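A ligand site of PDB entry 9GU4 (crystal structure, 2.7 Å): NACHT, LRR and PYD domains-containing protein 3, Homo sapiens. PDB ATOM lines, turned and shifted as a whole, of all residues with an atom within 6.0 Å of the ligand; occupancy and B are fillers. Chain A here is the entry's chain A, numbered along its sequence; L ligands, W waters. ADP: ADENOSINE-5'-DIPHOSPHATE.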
ATOM      1  N   ARG A  38      -8.009  16.145  -4.033  1.00  0.00           N
ATOM      2  CA  ARG A  38      -9.449  15.883  -4.155  1.00  0.00           C
ATOM      3  C   ARG A  38     -10.284  16.279  -2.939  1.00  0.00           C
ATOM      4  O   ARG A  38     -11.511  16.260  -3.038  1.00  0.00           O
ATOM      5  CB  ARG A  38      -9.745  14.421  -4.548  1.00  0.00           C
ATOM      6  CG  ARG A  38     -10.858  14.283  -5.581  1.00  0.00           C
ATOM      7  CD  ARG A  38     -11.505  12.938  -5.422  1.00  0.00           C
ATOM      8  NE  ARG A  38     -11.043  11.975  -6.425  1.00  0.00           N
ATOM      9  CZ  ARG A  38     -11.059  10.654  -6.249  1.00  0.00           C
ATOM     10  NH1 ARG A  38     -11.451  10.127  -5.099  1.00  0.00           N
ATOM     11  NH2 ARG A  38     -10.642   9.856  -7.225  1.00  0.00           N
ATOM     12  N   TYR A  39      -9.640  16.684  -1.826  1.00  0.00           N
ATOM     13  CA  TYR A  39     -10.403  17.122  -0.650  1.00  0.00           C
ATOM     14  C   TYR A  39     -11.233  18.362  -0.974  1.00  0.00           C
ATOM     15  O   TYR A  39     -10.681  19.410  -1.309  1.00  0.00           O
ATOM     16  CB  TYR A  39      -9.498  17.384   0.577  1.00  0.00           C
ATOM     17  CG  TYR A  39     -10.269  17.936   1.753  1.00  0.00           C
ATOM     18  CD1 TYR A  39     -11.078  17.117   2.515  1.00  0.00           C
ATOM     19  CD2 TYR A  39     -10.257  19.290   2.037  1.00  0.00           C
ATOM     20  CE1 TYR A  39     -11.844  17.632   3.560  1.00  0.00           C
ATOM     21  CE2 TYR A  39     -11.033  19.817   3.065  1.00  0.00           C
ATOM     22  CZ  TYR A  39     -11.822  18.985   3.831  1.00  0.00           C
ATOM     23  OH  TYR A  39     -12.585  19.497   4.848  1.00  0.00           O
ATOM     24  N   THR A  40     -12.560  18.230  -0.899  1.00  0.00           N
ATOM     25  CA  THR A  40     -13.479  19.331  -1.144  1.00  0.00           C
ATOM     26  C   THR A  40     -14.067  19.784   0.190  1.00  0.00           C
ATOM     27  O   THR A  40     -14.379  18.946   1.033  1.00  0.00           O
ATOM     28  CB  THR A  40     -14.522  18.932  -2.191  1.00  0.00           C
ATOM     29  OG1 THR A  40     -13.834  18.573  -3.383  1.00  0.00           O
ATOM     30  CG2 THR A  40     -15.517  20.037  -2.487  1.00  0.00           C
ATOM     31  N   ARG A  41     -14.177  21.095   0.410  1.00  0.00           N
ATOM     32  CA  ARG A  41     -14.683  21.655   1.654  1.00  0.00           C
ATOM     33  C   ARG A  41     -16.003  21.056   2.112  1.00  0.00           C
ATOM     34  O   ARG A  41     -16.949  20.936   1.329  1.00  0.00           O
ATOM     35  CB  ARG A  41     -14.799  23.184   1.548  1.00  0.00           C
ATOM     36  CG  ARG A  41     -14.892  23.921   2.871  1.00  0.00           C
ATOM     37  CD  ARG A  41     -15.318  25.379   2.685  1.00  0.00           C
ATOM     38  NE  ARG A  41     -14.332  26.143   1.911  1.00  0.00           N
ATOM     39  CZ  ARG A  41     -14.610  27.268   1.248  1.00  0.00           C
ATOM     40  NH1 ARG A  41     -15.845  27.769   1.268  1.00  0.00           N
ATOM     41  NH2 ARG A  41     -13.656  27.907   0.578  1.00  0.00           N
ATOM     42  N   LEU A  42     -16.051  20.640   3.377  1.00  0.00           N
ATOM     43  CA  LEU A  42     -17.238  20.082   4.000  1.00  0.00           C
ATOM     44  C   LEU A  42     -17.939  21.175   4.779  1.00  0.00           C
ATOM     45  O   LEU A  42     -17.279  22.008   5.402  1.00  0.00           O
ATOM     46  CB  LEU A  42     -16.865  18.933   4.954  1.00  0.00           C
ATOM     47  CG  LEU A  42     -16.404  17.655   4.301  1.00  0.00           C
ATOM     48  CD1 LEU A  42     -15.998  16.674   5.325  1.00  0.00           C
ATOM     49  CD2 LEU A  42     -17.502  17.049   3.459  1.00  0.00           C
ATOM     50  N   GLY A  97     -22.191  12.983  11.794  1.00  0.00           N
ATOM     51  CA  GLY A  97     -22.408  12.956  10.359  1.00  0.00           C
ATOM     52  C   GLY A  97     -23.010  11.673   9.879  1.00  0.00           C
ATOM     53  O   GLY A  97     -22.747  10.600  10.442  1.00  0.00           O
ATOM     54  N   ALA A  98     -23.824  11.750   8.823  1.00  0.00           N
ATOM     55  CA  ALA A  98     -24.442  10.567   8.230  1.00  0.00           C
ATOM     56  C   ALA A  98     -23.372   9.678   7.551  1.00  0.00           C
ATOM     57  O   ALA A  98     -22.235  10.137   7.320  1.00  0.00           O
ATOM     58  CB  ALA A  98     -25.497  11.006   7.223  1.00  0.00           C
ATOM     59  N   ALA A  99     -23.699   8.410   7.247  1.00  0.00           N
ATOM     60  CA  ALA A  99     -22.734   7.514   6.623  1.00  0.00           C
ATOM     61  C   ALA A  99     -22.275   8.072   5.268  1.00  0.00           C
ATOM     62  O   ALA A  99     -23.090   8.614   4.532  1.00  0.00           O
ATOM     63  CB  ALA A  99     -23.368   6.144   6.443  1.00  0.00           C
ATOM     64  N   GLY A 100     -20.973   8.068   5.020  1.00  0.00           N
ATOM     65  CA  GLY A 100     -20.433   8.602   3.791  1.00  0.00           C
ATOM     66  C   GLY A 100     -20.300  10.107   3.727  1.00  0.00           C
ATOM     67  O   GLY A 100     -19.861  10.647   2.716  1.00  0.00           O
ATOM     68  N   ILE A 101     -20.650  10.815   4.814  1.00  0.00           N
ATOM     69  CA  ILE A 101     -20.562  12.285   4.835  1.00  0.00           C
ATOM     70  C   ILE A 101     -19.119  12.805   4.842  1.00  0.00           C
ATOM     71  O   ILE A 101     -18.896  13.968   4.497  1.00  0.00           O
ATOM     72  CB  ILE A 101     -21.396  12.915   5.981  1.00  0.00           C
ATOM     73  CG1 ILE A 101     -22.078  14.213   5.530  1.00  0.00           C
ATOM     74  CG2 ILE A 101     -20.593  13.115   7.269  1.00  0.00           C
ATOM     75  CD1 ILE A 101     -23.041  14.066   4.406  1.00  0.00           C
ATOM     76  N   GLY A 102     -18.151  11.966   5.234  1.00  0.00           N
ATOM     77  CA  GLY A 102     -16.749  12.361   5.230  1.00  0.00           C
ATOM     78  C   GLY A 102     -16.158  12.622   6.597  1.00  0.00           C
ATOM     79  O   GLY A 102     -15.338  13.515   6.750  1.00  0.00           O
ATOM     80  N   LYS A 103     -16.548  11.819   7.593  1.00  0.00           N
ATOM     81  CA  LYS A 103     -15.998  11.961   8.941  1.00  0.00           C
ATOM     82  C   LYS A 103     -14.529  11.546   8.935  1.00  0.00           C
ATOM     83  O   LYS A 103     -13.707  12.230   9.548  1.00  0.00           O
ATOM     84  CB  LYS A 103     -16.809  11.142   9.946  1.00  0.00           C
ATOM     85  CG  LYS A 103     -18.226  11.654  10.082  1.00  0.00           C
ATOM     86  CD  LYS A 103     -18.994  10.962  11.178  1.00  0.00           C
ATOM     87  CE  LYS A 103     -19.287   9.535  10.838  1.00  0.00           C
ATOM     88  NZ  LYS A 103     -20.058   9.411   9.573  1.00  0.00           N
ATOM     89  N   THR A 104     -14.187  10.468   8.219  1.00  0.00           N
ATOM     90  CA  THR A 104     -12.814   9.978   8.112  1.00  0.00           C
ATOM     91  C   THR A 104     -11.956  10.919   7.269  1.00  0.00           C
ATOM     92  O   THR A 104     -10.798  11.178   7.620  1.00  0.00           O
ATOM     93  CB  THR A 104     -12.806   8.558   7.558  1.00  0.00           C
ATOM     94  OG1 THR A 104     -13.438   7.699   8.500  1.00  0.00           O
ATOM     95  CG2 THR A 104     -11.408   8.038   7.300  1.00  0.00           C
ATOM     96  N   ILE A 105     -12.525  11.448   6.172  1.00  0.00           N
ATOM     97  CA  ILE A 105     -11.766  12.376   5.328  1.00  0.00           C
ATOM     98  C   ILE A 105     -11.493  13.673   6.088  1.00  0.00           C
ATOM     99  O   ILE A 105     -10.393  14.229   5.971  1.00  0.00           O
ATOM    100  CB  ILE A 105     -12.407  12.581   3.946  1.00  0.00           C
ATOM    101  CG1 ILE A 105     -12.601  11.244   3.234  1.00  0.00           C
ATOM    102  CG2 ILE A 105     -11.569  13.534   3.100  1.00  0.00           C
ATOM    103  CD1 ILE A 105     -11.389  10.434   3.033  1.00  0.00           C
ATOM    104  N   LEU A 106     -12.437  14.112   6.938  1.00  0.00           N
ATOM    105  CA  LEU A 106     -12.223  15.306   7.754  1.00  0.00           C
ATOM    106  C   LEU A 106     -11.167  15.065   8.817  1.00  0.00           C
ATOM    107  O   LEU A 106     -10.285  15.908   8.996  1.00  0.00           O
ATOM    108  CB  LEU A 106     -13.523  15.784   8.392  1.00  0.00           C
ATOM    109  CG  LEU A 106     -13.441  17.184   8.971  1.00  0.00           C
ATOM    110  CD1 LEU A 106     -13.089  18.209   7.882  1.00  0.00           C
ATOM    111  CD2 LEU A 106     -14.719  17.563   9.658  1.00  0.00           C
ATOM    112  N   ASP A 173     -11.838   8.637  15.427  1.00  0.00           N
ATOM    113  CA  ASP A 173     -12.659   8.575  14.222  1.00  0.00           C
ATOM    114  C   ASP A 173     -13.592   7.371  14.214  1.00  0.00           C
ATOM    115  O   ASP A 173     -13.141   6.233  14.324  1.00  0.00           O
ATOM    116  CB  ASP A 173     -11.790   8.617  12.960  1.00  0.00           C
ATOM    117  CG  ASP A 173     -12.532   8.433  11.647  1.00  0.00           C
ATOM    118  OD1 ASP A 173     -13.701   8.887  11.543  1.00  0.00           O
ATOM    119  OD2 ASP A 173     -11.951   7.821  10.724  1.00  0.00           O
ATOM    120  N   GLU A 177     -18.409   2.897  15.103  1.00  0.00           N
ATOM    121  CA  GLU A 177     -17.779   1.740  14.488  1.00  0.00           C
ATOM    122  C   GLU A 177     -16.957   0.907  15.480  1.00  0.00           C
ATOM    123  O   GLU A 177     -16.156   0.096  15.045  1.00  0.00           O
ATOM    124  CB  GLU A 177     -16.912   2.169  13.290  1.00  0.00           C
ATOM    125  CG  GLU A 177     -17.723   2.840  12.196  1.00  0.00           C
ATOM    126  CD  GLU A 177     -16.943   3.259  10.961  1.00  0.00           C
ATOM    127  OE1 GLU A 177     -15.693   3.193  10.993  1.00  0.00           O
ATOM    128  OE2 GLU A 177     -17.605   3.674   9.975  1.00  0.00           O
ATOM    129  N   PHE A 244     -21.497  18.185   1.284  1.00  0.00           N
ATOM    130  CA  PHE A 244     -21.220  19.122   0.212  1.00  0.00           C
ATOM    131  C   PHE A 244     -22.342  20.117  -0.049  1.00  0.00           C
ATOM    132  O   PHE A 244     -23.518  19.742  -0.110  1.00  0.00           O
ATOM    133  CB  PHE A 244     -20.907  18.358  -1.086  1.00  0.00           C
ATOM    134  CG  PHE A 244     -19.582  17.622  -1.149  1.00  0.00           C
ATOM    135  CD1 PHE A 244     -18.547  17.968  -0.297  1.00  0.00           C
ATOM    136  CD2 PHE A 244     -19.366  16.638  -2.088  1.00  0.00           C
ATOM    137  CE1 PHE A 244     -17.328  17.310  -0.365  1.00  0.00           C
ATOM    138  CE2 PHE A 244     -18.137  15.993  -2.171  1.00  0.00           C
ATOM    139  CZ  PHE A 244     -17.122  16.332  -1.314  1.00  0.00           C
ATOM    140  N   TYR A 252     -16.488  19.051  -6.707  1.00  0.00           N
ATOM    141  CA  TYR A 252     -16.072  17.632  -6.669  1.00  0.00           C
ATOM    142  C   TYR A 252     -16.083  17.031  -8.054  1.00  0.00           C
ATOM    143  O   TYR A 252     -15.145  16.335  -8.432  1.00  0.00           O
ATOM    144  CB  TYR A 252     -16.956  16.793  -5.733  1.00  0.00           C
ATOM    145  CG  TYR A 252     -16.440  15.372  -5.578  1.00  0.00           C
ATOM    146  CD1 TYR A 252     -16.800  14.373  -6.488  1.00  0.00           C
ATOM    147  CD2 TYR A 252     -15.596  15.031  -4.539  1.00  0.00           C
ATOM    148  CE1 TYR A 252     -16.279  13.090  -6.376  1.00  0.00           C
ATOM    149  CE2 TYR A 252     -15.097  13.742  -4.407  1.00  0.00           C
ATOM    150  CZ  TYR A 252     -15.449  12.771  -5.320  1.00  0.00           C
ATOM    151  OH  TYR A 252     -14.950  11.496  -5.190  1.00  0.00           O
ATOM    152  N   PRO A 283     -20.790  13.158   0.229  1.00  0.00           N
ATOM    153  CA  PRO A 283     -19.602  12.963  -0.609  1.00  0.00           C
ATOM    154  C   PRO A 283     -19.389  11.514  -1.075  1.00  0.00           C
ATOM    155  O   PRO A 283     -18.803  11.308  -2.137  1.00  0.00           O
ATOM    156  CB  PRO A 283     -18.471  13.449   0.293  1.00  0.00           C
ATOM    157  CG  PRO A 283     -19.137  14.420   1.218  1.00  0.00           C
ATOM    158  CD  PRO A 283     -20.429  13.775   1.526  1.00  0.00           C
ATOM    159  N   LEU A 284     -19.893  10.519  -0.326  1.00  0.00           N
ATOM    160  CA  LEU A 284     -19.787   9.126  -0.752  1.00  0.00           C
ATOM    161  C   LEU A 284     -20.622   8.920  -2.020  1.00  0.00           C
ATOM    162  O   LEU A 284     -20.140   8.294  -2.960  1.00  0.00           O
ATOM    163  CB  LEU A 284     -20.224   8.141   0.353  1.00  0.00           C
ATOM    164  CG  LEU A 284     -20.206   6.661  -0.043  1.00  0.00           C
ATOM    165  CD1 LEU A 284     -18.836   6.197  -0.475  1.00  0.00           C
ATOM    166  CD2 LEU A 284     -20.714   5.815   1.068  1.00  0.00           C
ATOM    167  N   TRP A 287     -18.746  10.249  -5.008  1.00  0.00           N
ATOM    168  CA  TRP A 287     -17.733   9.311  -5.472  1.00  0.00           C
ATOM    169  C   TRP A 287     -18.356   8.123  -6.223  1.00  0.00           C
ATOM    170  O   TRP A 287     -17.921   7.811  -7.324  1.00  0.00           O
ATOM    171  CB  TRP A 287     -16.872   8.824  -4.294  1.00  0.00           C
ATOM    172  CG  TRP A 287     -15.765   7.893  -4.685  1.00  0.00           C
ATOM    173  CD1 TRP A 287     -14.505   8.228  -5.062  1.00  0.00           C
ATOM    174  CD2 TRP A 287     -15.819   6.458  -4.664  1.00  0.00           C
ATOM    175  NE1 TRP A 287     -13.776   7.089  -5.339  1.00  0.00           N
ATOM    176  CE2 TRP A 287     -14.559   5.988  -5.092  1.00  0.00           C
ATOM    177  CE3 TRP A 287     -16.819   5.524  -4.358  1.00  0.00           C
ATOM    178  CZ2 TRP A 287     -14.274   4.629  -5.203  1.00  0.00           C
ATOM    179  CZ3 TRP A 287     -16.541   4.187  -4.516  1.00  0.00           C
ATOM    180  CH2 TRP A 287     -15.277   3.751  -4.904  1.00  0.00           C
ATOM    181  N   ILE A 392     -15.085  -0.976   0.777  1.00  0.00           N
ATOM    182  CA  ILE A 392     -14.768   0.466   0.632  1.00  0.00           C
ATOM    183  C   ILE A 392     -15.495   1.342   1.633  1.00  0.00           C
ATOM    184  O   ILE A 392     -14.942   2.341   2.090  1.00  0.00           O
ATOM    185  CB  ILE A 392     -14.938   1.050  -0.789  1.00  0.00           C
ATOM    186  CG1 ILE A 392     -16.013   0.337  -1.588  1.00  0.00           C
ATOM    187  CG2 ILE A 392     -13.616   1.117  -1.529  1.00  0.00           C
ATOM    188  CD1 ILE A 392     -16.561   1.169  -2.596  1.00  0.00           C
ATOM    189  N   HIS A 393     -16.719   0.976   1.973  1.00  0.00           N
ATOM    190  CA  HIS A 393     -17.485   1.705   2.958  1.00  0.00           C
ATOM    191  C   HIS A 393     -18.349   0.752   3.766  1.00  0.00           C
ATOM    192  O   HIS A 393     -18.666  -0.351   3.337  1.00  0.00           O
ATOM    193  CB  HIS A 393     -18.301   2.847   2.339  1.00  0.00           C
ATOM    194  CG  HIS A 393     -18.736   3.868   3.339  1.00  0.00           C
ATOM    195  ND1 HIS A 393     -19.975   3.804   3.944  1.00  0.00           N
ATOM    196  CD2 HIS A 393     -18.060   4.923   3.845  1.00  0.00           C
ATOM    197  CE1 HIS A 393     -20.022   4.820   4.775  1.00  0.00           C
ATOM    198  NE2 HIS A 393     -18.890   5.525   4.752  1.00  0.00           N
ATOM    199  N   MET A 394     -18.712   1.182   4.975  1.00  0.00           N
ATOM    200  CA  MET A 394     -19.557   0.425   5.863  1.00  0.00           C
ATOM    201  C   MET A 394     -20.948   0.159   5.203  1.00  0.00           C
ATOM    202  O   MET A 394     -21.490  -0.925   5.343  1.00  0.00           O
ATOM    203  CB  MET A 394     -19.594   1.151   7.243  1.00  0.00           C
ATOM    204  CG  MET A 394     -20.941   1.238   7.913  1.00  0.00           C
ATOM    205  SD  MET A 394     -21.875   2.719   7.445  1.00  0.00           S
ATOM    206  CE  MET A 394     -23.488   2.165   7.774  1.00  0.00           C
HETATM  207  PB  ADP L   1     -17.818   8.513   6.924  1.00  0.00           P
HETATM  208  O1B ADP L   1     -16.573   8.327   7.757  1.00  0.00           O
HETATM  209  O2B ADP L   1     -18.643   9.712   7.335  1.00  0.00           O
HETATM  210  O3B ADP L   1     -18.648   7.249   6.834  1.00  0.00           O
HETATM  211  PA  ADP L   1     -15.787   8.836   4.753  1.00  0.00           P
HETATM  212  O1A ADP L   1     -15.025  10.019   5.211  1.00  0.00           O
HETATM  213  O2A ADP L   1     -15.197   7.486   4.929  1.00  0.00           O
HETATM  214  O3A ADP L   1     -17.231   8.856   5.443  1.00  0.00           O
HETATM  215  O5' ADP L   1     -16.148   9.125   3.218  1.00  0.00           O
HETATM  216  C5' ADP L   1     -16.287   8.060   2.252  1.00  0.00           C
HETATM  217  C4' ADP L   1     -15.891   8.553   0.870  1.00  0.00           C
HETATM  218  O4' ADP L   1     -16.426   9.868   0.667  1.00  0.00           O
HETATM  219  C3' ADP L   1     -14.387   8.682   0.620  1.00  0.00           C
HETATM  220  O3' ADP L   1     -13.853   7.475   0.102  1.00  0.00           O
HETATM  221  C2' ADP L   1     -14.300   9.820  -0.415  1.00  0.00           C
HETATM  222  O2' ADP L   1     -14.298   9.436  -1.781  1.00  0.00           O
HETATM  223  C1' ADP L   1     -15.542  10.653  -0.119  1.00  0.00           C
HETATM  224  N9  ADP L   1     -15.261  11.869   0.615  1.00  0.00           N
HETATM  225  C8  ADP L   1     -15.730  12.170   1.871  1.00  0.00           C
HETATM  226  N7  ADP L   1     -15.457  13.394   2.254  1.00  0.00           N
HETATM  227  C5  ADP L   1     -14.772  13.934   1.189  1.00  0.00           C
HETATM  228  C6  ADP L   1     -14.254  15.219   0.938  1.00  0.00           C
HETATM  229  N6  ADP L   1     -14.354  16.230   1.815  1.00  0.00           N
HETATM  230  N1  ADP L   1     -13.656  15.447  -0.251  1.00  0.00           N
HETATM  231  C2  ADP L   1     -13.596  14.447  -1.133  1.00  0.00           C
HETATM  232  N3  ADP L   1     -14.053  13.192  -1.022  1.00  0.00           N
HETATM  233  C4  ADP L   1     -14.634  13.001   0.171  1.00  0.00           C
HETATM  234  O   HOH W   1     -13.821   4.987  -1.222  1.00  0.00           O
HETATM  235  O   HOH W   2     -20.345   6.590   9.020  1.00  0.00           O
HETATM  236  O   HOH W   3     -13.157   6.740   3.237  1.00  0.00           O
HETATM  237  O   HOH W   4     -15.541   6.997  10.099  1.00  0.00           O
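Residues that only touch the ligand: Arg 38 (3.4 Å), Tyr 39 (3.4 Å), Pro 283 (3.4 Å), Trp 287 (3.5 Å), Leu 42 (3.5 Å), Tyr 252 (3.6 Å), Ala 98 (3.6 Å), Leu 284 (3.7 Å) and Phe 244 (3.7 Å).
Hydrophobic or aromatic side chains within 4 Å of the ligand: Tyr 39, Leu 42, Ile 101, Ile 105, Phe 244, Tyr 252, Pro 283, Trp 287 and His 393.
17 residues have an atom within 4 Å of the ligand: Arg 38, Tyr 39, Thr 40, Leu 42, Ala 98, Gly 100, Ile 101, Gly 102, Lys 103, Thr 104, Ile 105, Phe 244, Tyr 252, Pro 283, Leu 284, Trp 287 and His 393.
The nearest printed residue that does not touch the ligand is Ala 99 (4.04 Å).
The backbone NH (N) of Lys 103 lies within hydrogen-bond range of an oxygen (O2B) of the ligand, at 3.0 Å.
NZ of Lys 103 is in salt-bridge range of O2B of the ligand (2.7 Å).
An oxygen (O3B) of the ligand sits at hydrogen-bond distance from a ring nitrogen (NE2) of His 393 (2.7 Å).
N of Thr 40 sits at hydrogen-bond distance from N1 of the ligand, at 3.1 Å.
O of Thr 40 lies within hydrogen-bond range of N6 of the ligand, 2.8 Å away.
O2B of the ligand is in hydrogen-bond range of N of Gly 102, 3.1 Å away.
N of Ile 105 is in hydrogen-bond range of O1A of the ligand (3.0 Å).
The backbone NH (N) of Gly 100 is in hydrogen-bond range of an oxygen (O3B) of the ligand.
An oxygen (O1A) of the ligand is in hydrogen-bond range of the backbone NH of Thr 104 (3.2 Å).
The side-chain hydroxyl (OG1) of Thr 104 is in hydrogen-bond range of an oxygen (O1B) of the ligand.
N of Ile 101 lies within hydrogen-bond range of O2B of the ligand, 3.4 Å away.
Water W2 bridges O3B of the ligand (2.8 Å) and NZ of Lys 103 (2.9 Å).
Water W4 lies within hydrogen-bond range of the side-chain hydroxyl of Thr 104, an oxygen (O1B) of the ligand and the side-chain carboxylate of Asp 173.
The side-chain amino group of Lys 103 is in hydrogen-bond range of the backbone carbonyl oxygen of Ala 98.
The side-chain amino group of Lys 103 lies within hydrogen-bond range of the backbone carbonyl oxygen of Gly 97, 3.1 Å away.
The backbone NH (N) of Gly 100 lies within hydrogen-bond range of a ring nitrogen (NE2) of His 393 (3.3 Å).
The side-chain hydroxyl (OG1) of Thr 40 sits at hydrogen-bond distance from the backbone carbonyl oxygen (O) of Arg 38, 3.3 Å away.
O of Gly 100 is in hydrogen-bond range of N of Leu 284 (3.0 Å).
OD2 of Asp 173 is in hydrogen-bond range of OG1 of Thr 104, at 2.7 Å.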
